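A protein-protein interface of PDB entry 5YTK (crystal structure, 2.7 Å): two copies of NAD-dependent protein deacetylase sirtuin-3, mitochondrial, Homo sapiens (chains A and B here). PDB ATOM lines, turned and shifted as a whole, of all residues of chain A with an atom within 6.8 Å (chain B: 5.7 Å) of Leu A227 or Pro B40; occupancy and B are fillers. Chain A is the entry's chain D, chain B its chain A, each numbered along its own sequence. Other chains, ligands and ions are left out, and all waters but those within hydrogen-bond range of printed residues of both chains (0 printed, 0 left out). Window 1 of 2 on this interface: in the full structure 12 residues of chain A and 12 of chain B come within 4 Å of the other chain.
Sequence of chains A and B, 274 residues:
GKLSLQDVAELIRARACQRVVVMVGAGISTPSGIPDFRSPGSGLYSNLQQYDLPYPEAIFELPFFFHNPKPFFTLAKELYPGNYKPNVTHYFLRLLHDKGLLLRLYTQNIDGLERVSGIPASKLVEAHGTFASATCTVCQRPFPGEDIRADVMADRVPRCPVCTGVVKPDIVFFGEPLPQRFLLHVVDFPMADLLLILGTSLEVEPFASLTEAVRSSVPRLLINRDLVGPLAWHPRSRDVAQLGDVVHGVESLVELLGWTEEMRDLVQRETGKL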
ATOM      1  N   LEU A 222      -4.574   7.005  13.201  1.00  0.00           N
ATOM      2  CA  LEU A 222      -3.407   7.456  13.947  1.00  0.00           C
ATOM      3  C   LEU A 222      -3.590   8.864  14.500  1.00  0.00           C
ATOM      4  O   LEU A 222      -3.816   9.807  13.749  1.00  0.00           O
ATOM      5  CB  LEU A 222      -2.161   7.413  13.068  1.00  0.00           C
ATOM      6  CG  LEU A 222      -0.901   8.015  13.691  1.00  0.00           C
ATOM      7  CD1 LEU A 222      -0.431   7.172  14.856  1.00  0.00           C
ATOM      8  CD2 LEU A 222       0.197   8.147  12.657  1.00  0.00           C
ATOM      9  N   ASN A 224      -1.271  11.231  16.402  1.00  0.00           N
ATOM     10  CA  ASN A 224       0.107  11.403  16.839  1.00  0.00           C
ATOM     11  C   ASN A 224       0.674  12.715  16.315  1.00  0.00           C
ATOM     12  O   ASN A 224       0.052  13.378  15.492  1.00  0.00           O
ATOM     13  CB  ASN A 224       0.963  10.223  16.370  1.00  0.00           C
ATOM     14  CG  ASN A 224       2.303  10.155  17.072  1.00  0.00           C
ATOM     15  OD1 ASN A 224       2.392  10.355  18.283  1.00  0.00           O
ATOM     16  ND2 ASN A 224       3.356   9.887  16.311  1.00  0.00           N
ATOM     17  N   ARG A 225       1.850  13.093  16.799  1.00  0.00           N
ATOM     18  CA  ARG A 225       2.512  14.293  16.311  1.00  0.00           C
ATOM     19  C   ARG A 225       2.957  14.134  14.863  1.00  0.00           C
ATOM     20  O   ARG A 225       2.773  15.032  14.043  1.00  0.00           O
ATOM     21  CB  ARG A 225       3.706  14.643  17.194  1.00  0.00           C
ATOM     22  CG  ARG A 225       4.408  15.917  16.779  1.00  0.00           C
ATOM     23  CD  ARG A 225       3.471  17.097  16.947  1.00  0.00           C
ATOM     24  NE  ARG A 225       3.055  17.279  18.333  1.00  0.00           N
ATOM     25  CZ  ARG A 225       2.152  18.172  18.725  1.00  0.00           C
ATOM     26  NH1 ARG A 225       1.572  18.962  17.831  1.00  0.00           N
ATOM     27  NH2 ARG A 225       1.825  18.269  20.006  1.00  0.00           N
ATOM     28  N   ASP A 226       3.538  12.981  14.549  1.00  0.00           N
ATOM     29  CA  ASP A 226       4.084  12.752  13.224  1.00  0.00           C
ATOM     30  C   ASP A 226       3.473  11.523  12.565  1.00  0.00           C
ATOM     31  O   ASP A 226       2.955  10.637  13.241  1.00  0.00           O
ATOM     32  CB  ASP A 226       5.600  12.594  13.306  1.00  0.00           C
ATOM     33  CG  ASP A 226       6.242  13.618  14.215  1.00  0.00           C
ATOM     34  OD1 ASP A 226       5.928  14.817  14.076  1.00  0.00           O
ATOM     35  OD2 ASP A 226       7.060  13.223  15.070  1.00  0.00           O
ATOM     36  N   LEU A 227       3.539  11.474  11.240  1.00  0.00           N
ATOM     37  CA  LEU A 227       3.190  10.269  10.505  1.00  0.00           C
ATOM     38  C   LEU A 227       4.469   9.527  10.144  1.00  0.00           C
ATOM     39  O   LEU A 227       5.056   9.759   9.089  1.00  0.00           O
ATOM     40  CB  LEU A 227       2.384  10.609   9.251  1.00  0.00           C
ATOM     41  CG  LEU A 227       2.073   9.467   8.280  1.00  0.00           C
ATOM     42  CD1 LEU A 227       1.226   8.404   8.951  1.00  0.00           C
ATOM     43  CD2 LEU A 227       1.397   9.985   7.022  1.00  0.00           C
ATOM     44  N   VAL A 228       4.920   8.657  11.043  1.00  0.00           N
ATOM     45  CA  VAL A 228       6.112   7.853  10.798  1.00  0.00           C
ATOM     46  C   VAL A 228       5.831   6.405  11.202  1.00  0.00           C
ATOM     47  O   VAL A 228       4.769   6.098  11.741  1.00  0.00           O
ATOM     48  CB  VAL A 228       7.355   8.389  11.570  1.00  0.00           C
ATOM     49  CG1 VAL A 228       8.644   7.996  10.855  1.00  0.00           C
ATOM     50  CG2 VAL A 228       7.307   9.898  11.709  1.00  0.00           C
ATOM     51  N   GLY A 229       6.787   5.521  10.943  1.00  0.00           N
ATOM     52  CA  GLY A 229       6.630   4.117  11.256  1.00  0.00           C
ATOM     53  C   GLY A 229       5.977   3.370  10.113  1.00  0.00           C
ATOM     54  O   GLY A 229       5.911   3.877   8.996  1.00  0.00           O
ATOM     55  N   LEU A 231       3.046   2.871   9.365  1.00  0.00           N
ATOM     56  CA  LEU A 231       1.883   3.544   8.816  1.00  0.00           C
ATOM     57  C   LEU A 231       2.269   4.465   7.669  1.00  0.00           C
ATOM     58  O   LEU A 231       1.485   4.691   6.748  1.00  0.00           O
ATOM     59  CB  LEU A 231       1.182   4.339   9.914  1.00  0.00           C
ATOM     60  CG  LEU A 231       0.241   3.551  10.822  1.00  0.00           C
ATOM     61  CD1 LEU A 231      -0.435   4.483  11.798  1.00  0.00           C
ATOM     62  CD2 LEU A 231      -0.785   2.808  10.004  1.00  0.00           C
ATOM     63  N   ALA A 232       3.490   4.982   7.721  1.00  0.00           N
ATOM     64  CA  ALA A 232       3.999   5.838   6.661  1.00  0.00           C
ATOM     65  C   ALA A 232       4.520   5.004   5.500  1.00  0.00           C
ATOM     66  O   ALA A 232       4.323   5.349   4.338  1.00  0.00           O
ATOM     67  CB  ALA A 232       5.094   6.745   7.194  1.00  0.00           C
ATOM     68  N   TRP A 233       5.188   3.904   5.825  1.00  0.00           N
ATOM     69  CA  TRP A 233       5.822   3.070   4.816  1.00  0.00           C
ATOM     70  C   TRP A 233       4.821   2.205   4.066  1.00  0.00           C
ATOM     71  O   TRP A 233       4.935   2.016   2.858  1.00  0.00           O
ATOM     72  CB  TRP A 233       6.889   2.183   5.447  1.00  0.00           C
ATOM     73  CG  TRP A 233       7.719   1.503   4.424  1.00  0.00           C
ATOM     74  CD1 TRP A 233       7.747   0.172   4.137  1.00  0.00           C
ATOM     75  CD2 TRP A 233       8.647   2.126   3.531  1.00  0.00           C
ATOM     76  NE1 TRP A 233       8.638  -0.074   3.122  1.00  0.00           N
ATOM     77  CE2 TRP A 233       9.205   1.114   2.734  1.00  0.00           C
ATOM     78  CE3 TRP A 233       9.061   3.447   3.331  1.00  0.00           C
ATOM     79  CZ2 TRP A 233      10.155   1.375   1.751  1.00  0.00           C
ATOM     80  CZ3 TRP A 233      10.003   3.706   2.359  1.00  0.00           C
ATOM     81  CH2 TRP A 233      10.541   2.676   1.581  1.00  0.00           C
ATOM     82  N   ALA A 241      -5.257   9.900   9.380  1.00  0.00           N
ATOM     83  CA  ALA A 241      -4.234  10.478  10.243  1.00  0.00           C
ATOM     84  C   ALA A 241      -4.645  11.820  10.837  1.00  0.00           C
ATOM     85  O   ALA A 241      -4.896  12.778  10.115  1.00  0.00           O
ATOM     86  CB  ALA A 241      -2.933  10.626   9.483  1.00  0.00           C
ATOM     87  N   LEU A 243      -2.849  14.275  12.668  1.00  0.00           N
ATOM     88  CA  LEU A 243      -1.548  14.749  13.116  1.00  0.00           C
ATOM     89  C   LEU A 243      -1.718  16.023  13.918  1.00  0.00           C
ATOM     90  O   LEU A 243      -2.664  16.776  13.709  1.00  0.00           O
ATOM     91  CB  LEU A 243      -0.603  14.981  11.937  1.00  0.00           C
ATOM     92  CG  LEU A 243      -0.371  13.787  11.014  1.00  0.00           C
ATOM     93  CD1 LEU A 243       0.694  14.111   9.979  1.00  0.00           C
ATOM     94  CD2 LEU A 243       0.020  12.564  11.833  1.00  0.00           C
ATOM     95  N   ASP B  36      15.489  12.850   3.186  1.00  0.00           N
ATOM     96  CA  ASP B  36      15.498  11.720   4.105  1.00  0.00           C
ATOM     97  C   ASP B  36      14.636  10.590   3.548  1.00  0.00           C
ATOM     98  O   ASP B  36      13.423  10.738   3.402  1.00  0.00           O
ATOM     99  CB  ASP B  36      15.005  12.141   5.489  1.00  0.00           C
ATOM    100  CG  ASP B  36      15.107  11.023   6.508  1.00  0.00           C
ATOM    101  OD1 ASP B  36      15.924  10.100   6.305  1.00  0.00           O
ATOM    102  OD2 ASP B  36      14.371  11.068   7.517  1.00  0.00           O
ATOM    103  N   ARG B  38      13.773   7.875   4.837  1.00  0.00           N
ATOM    104  CA  ARG B  38      12.934   7.245   5.849  1.00  0.00           C
ATOM    105  C   ARG B  38      11.636   8.016   6.034  1.00  0.00           C
ATOM    106  O   ARG B  38      10.631   7.462   6.476  1.00  0.00           O
ATOM    107  CB  ARG B  38      13.675   7.163   7.185  1.00  0.00           C
ATOM    108  CG  ARG B  38      14.999   6.423   7.136  1.00  0.00           C
ATOM    109  CD  ARG B  38      15.683   6.402   8.499  1.00  0.00           C
ATOM    110  NE  ARG B  38      16.090   7.739   8.931  1.00  0.00           N
ATOM    111  CZ  ARG B  38      15.441   8.477   9.829  1.00  0.00           C
ATOM    112  NH1 ARG B  38      15.891   9.684  10.149  1.00  0.00           N
ATOM    113  NH2 ARG B  38      14.346   8.010  10.415  1.00  0.00           N
ATOM    114  N   SER B  39      11.665   9.297   5.689  1.00  0.00           N
ATOM    115  CA  SER B  39      10.532  10.179   5.932  1.00  0.00           C
ATOM    116  C   SER B  39       9.692  10.376   4.679  1.00  0.00           C
ATOM    117  O   SER B  39      10.224  10.687   3.614  1.00  0.00           O
ATOM    118  CB  SER B  39      11.013  11.533   6.456  1.00  0.00           C
ATOM    119  OG  SER B  39       9.963  12.483   6.443  1.00  0.00           O
ATOM    120  N   PRO B  40       8.370  10.188   4.803  1.00  0.00           N
ATOM    121  CA  PRO B  40       7.452  10.403   3.681  1.00  0.00           C
ATOM    122  C   PRO B  40       7.427  11.865   3.263  1.00  0.00           C
ATOM    123  O   PRO B  40       7.678  12.740   4.089  1.00  0.00           O
ATOM    124  CB  PRO B  40       6.096   9.971   4.244  1.00  0.00           C
ATOM    125  CG  PRO B  40       6.239  10.094   5.721  1.00  0.00           C
ATOM    126  CD  PRO B  40       7.664   9.761   6.022  1.00  0.00           C
ATOM    127  N   GLY B  41       7.136  12.124   1.993  1.00  0.00           N
ATOM    128  CA  GLY B  41       7.059  13.488   1.504  1.00  0.00           C
ATOM    129  C   GLY B  41       8.086  13.807   0.437  1.00  0.00           C
ATOM    130  O   GLY B  41       7.947  14.788  -0.290  1.00  0.00           O
ATOM    131  N   SER B  42       9.115  12.974   0.332  1.00  0.00           N
ATOM    132  CA  SER B  42      10.132  13.167  -0.691  1.00  0.00           C
ATOM    133  C   SER B  42       9.871  12.262  -1.887  1.00  0.00           C
ATOM    134  O   SER B  42       9.215  11.229  -1.763  1.00  0.00           O
ATOM    135  CB  SER B  42      11.525  12.920  -0.109  1.00  0.00           C
ATOM    136  OG  SER B  42      11.505  11.872   0.844  1.00  0.00           O
ATOM    137  N   TYR B  45      11.339   8.773  -1.439  1.00  0.00           N
ATOM    138  CA  TYR B  45      10.481   7.933  -0.613  1.00  0.00           C
ATOM    139  C   TYR B  45       9.394   7.298  -1.477  1.00  0.00           C
ATOM    140  O   TYR B  45       9.155   6.087  -1.429  1.00  0.00           O
ATOM    141  CB  TYR B  45       9.869   8.778   0.502  1.00  0.00           C
ATOM    142  CG  TYR B  45       9.160   8.016   1.593  1.00  0.00           C
ATOM    143  CD1 TYR B  45       7.825   7.662   1.479  1.00  0.00           C
ATOM    144  CD2 TYR B  45       9.830   7.676   2.759  1.00  0.00           C
ATOM    145  CE1 TYR B  45       7.188   6.976   2.494  1.00  0.00           C
ATOM    146  CE2 TYR B  45       9.203   6.992   3.774  1.00  0.00           C
ATOM    147  CZ  TYR B  45       7.883   6.643   3.638  1.00  0.00           C
ATOM    148  OH  TYR B  45       7.263   5.960   4.660  1.00  0.00           O
ATOM    149  N   GLN B  49       8.710   3.372  -2.446  1.00  0.00           N
ATOM    150  CA  GLN B  49       7.477   2.660  -2.113  1.00  0.00           C
ATOM    151  C   GLN B  49       7.055   1.690  -3.216  1.00  0.00           C
ATOM    152  O   GLN B  49       6.215   0.821  -2.996  1.00  0.00           O
ATOM    153  CB  GLN B  49       6.342   3.639  -1.840  1.00  0.00           C
ATOM    154  CG  GLN B  49       6.429   4.333  -0.508  1.00  0.00           C
ATOM    155  CD  GLN B  49       5.145   5.053  -0.171  1.00  0.00           C
ATOM    156  OE1 GLN B  49       5.041   5.709   0.862  1.00  0.00           O
ATOM    157  NE2 GLN B  49       4.153   4.929  -1.046  1.00  0.00           N
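Of the 12 printed residues of chain A, 3 touch a printed residue of chain B. Printed residues of chain A that touch a printed residue of chain B: Leu A227, Ala A232 and Trp A233. Of the 8 printed residues of chain B, 3 touch a printed residue of chain A. Among the printed residues, 5 pairs touch across the chains. Among the printed residues, no Asp or Glu carboxylate lies within 4 Å of a Lys or Arg side-chain nitrogen of the other chain.
O of Ala A232 is in hydrogen-bond range of OH of Tyr B45. OH of Tyr B45 lies within hydrogen-bond range of N of Trp A233.
O of Leu A227 touches CG of Pro B40 (3.6 Å). CG of Pro B40 touches CB of Ala A232, at 3.8 Å. Ala A232 touches Gln B49 (O to OE1, 3.6 Å).
No position is printed for both chains. Of the 5 pairs that touch across the chains among the printed residues, none has its exchanged pair printed and touching as well.
Of the printed residues of chain A, Gln B49 touches Ala A232 (3.6 Å). Printed residues of chain A within 4 Å of Tyr B45: Ala A232 (3.0 Å) and Trp A233 (3.1 Å). Of the printed residues of chain B, Trp A233 touches Tyr B45. Of the printed residues of chain B, Ala A232 touches Pro B40 (3.8 Å), Tyr B45 (3.0 Å) and Gln B49 (3.6 Å). Gly A229 touches none of the printed residues of chain B. Val A228 touches none of the printed residues of chain B. The nearest printed residue of chain B that does not touch Leu A227 is Ser B39 (6.2 Å). The nearest printed residue of chain B that does not touch Trp A233 is Gln B49 (4.2 Å).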
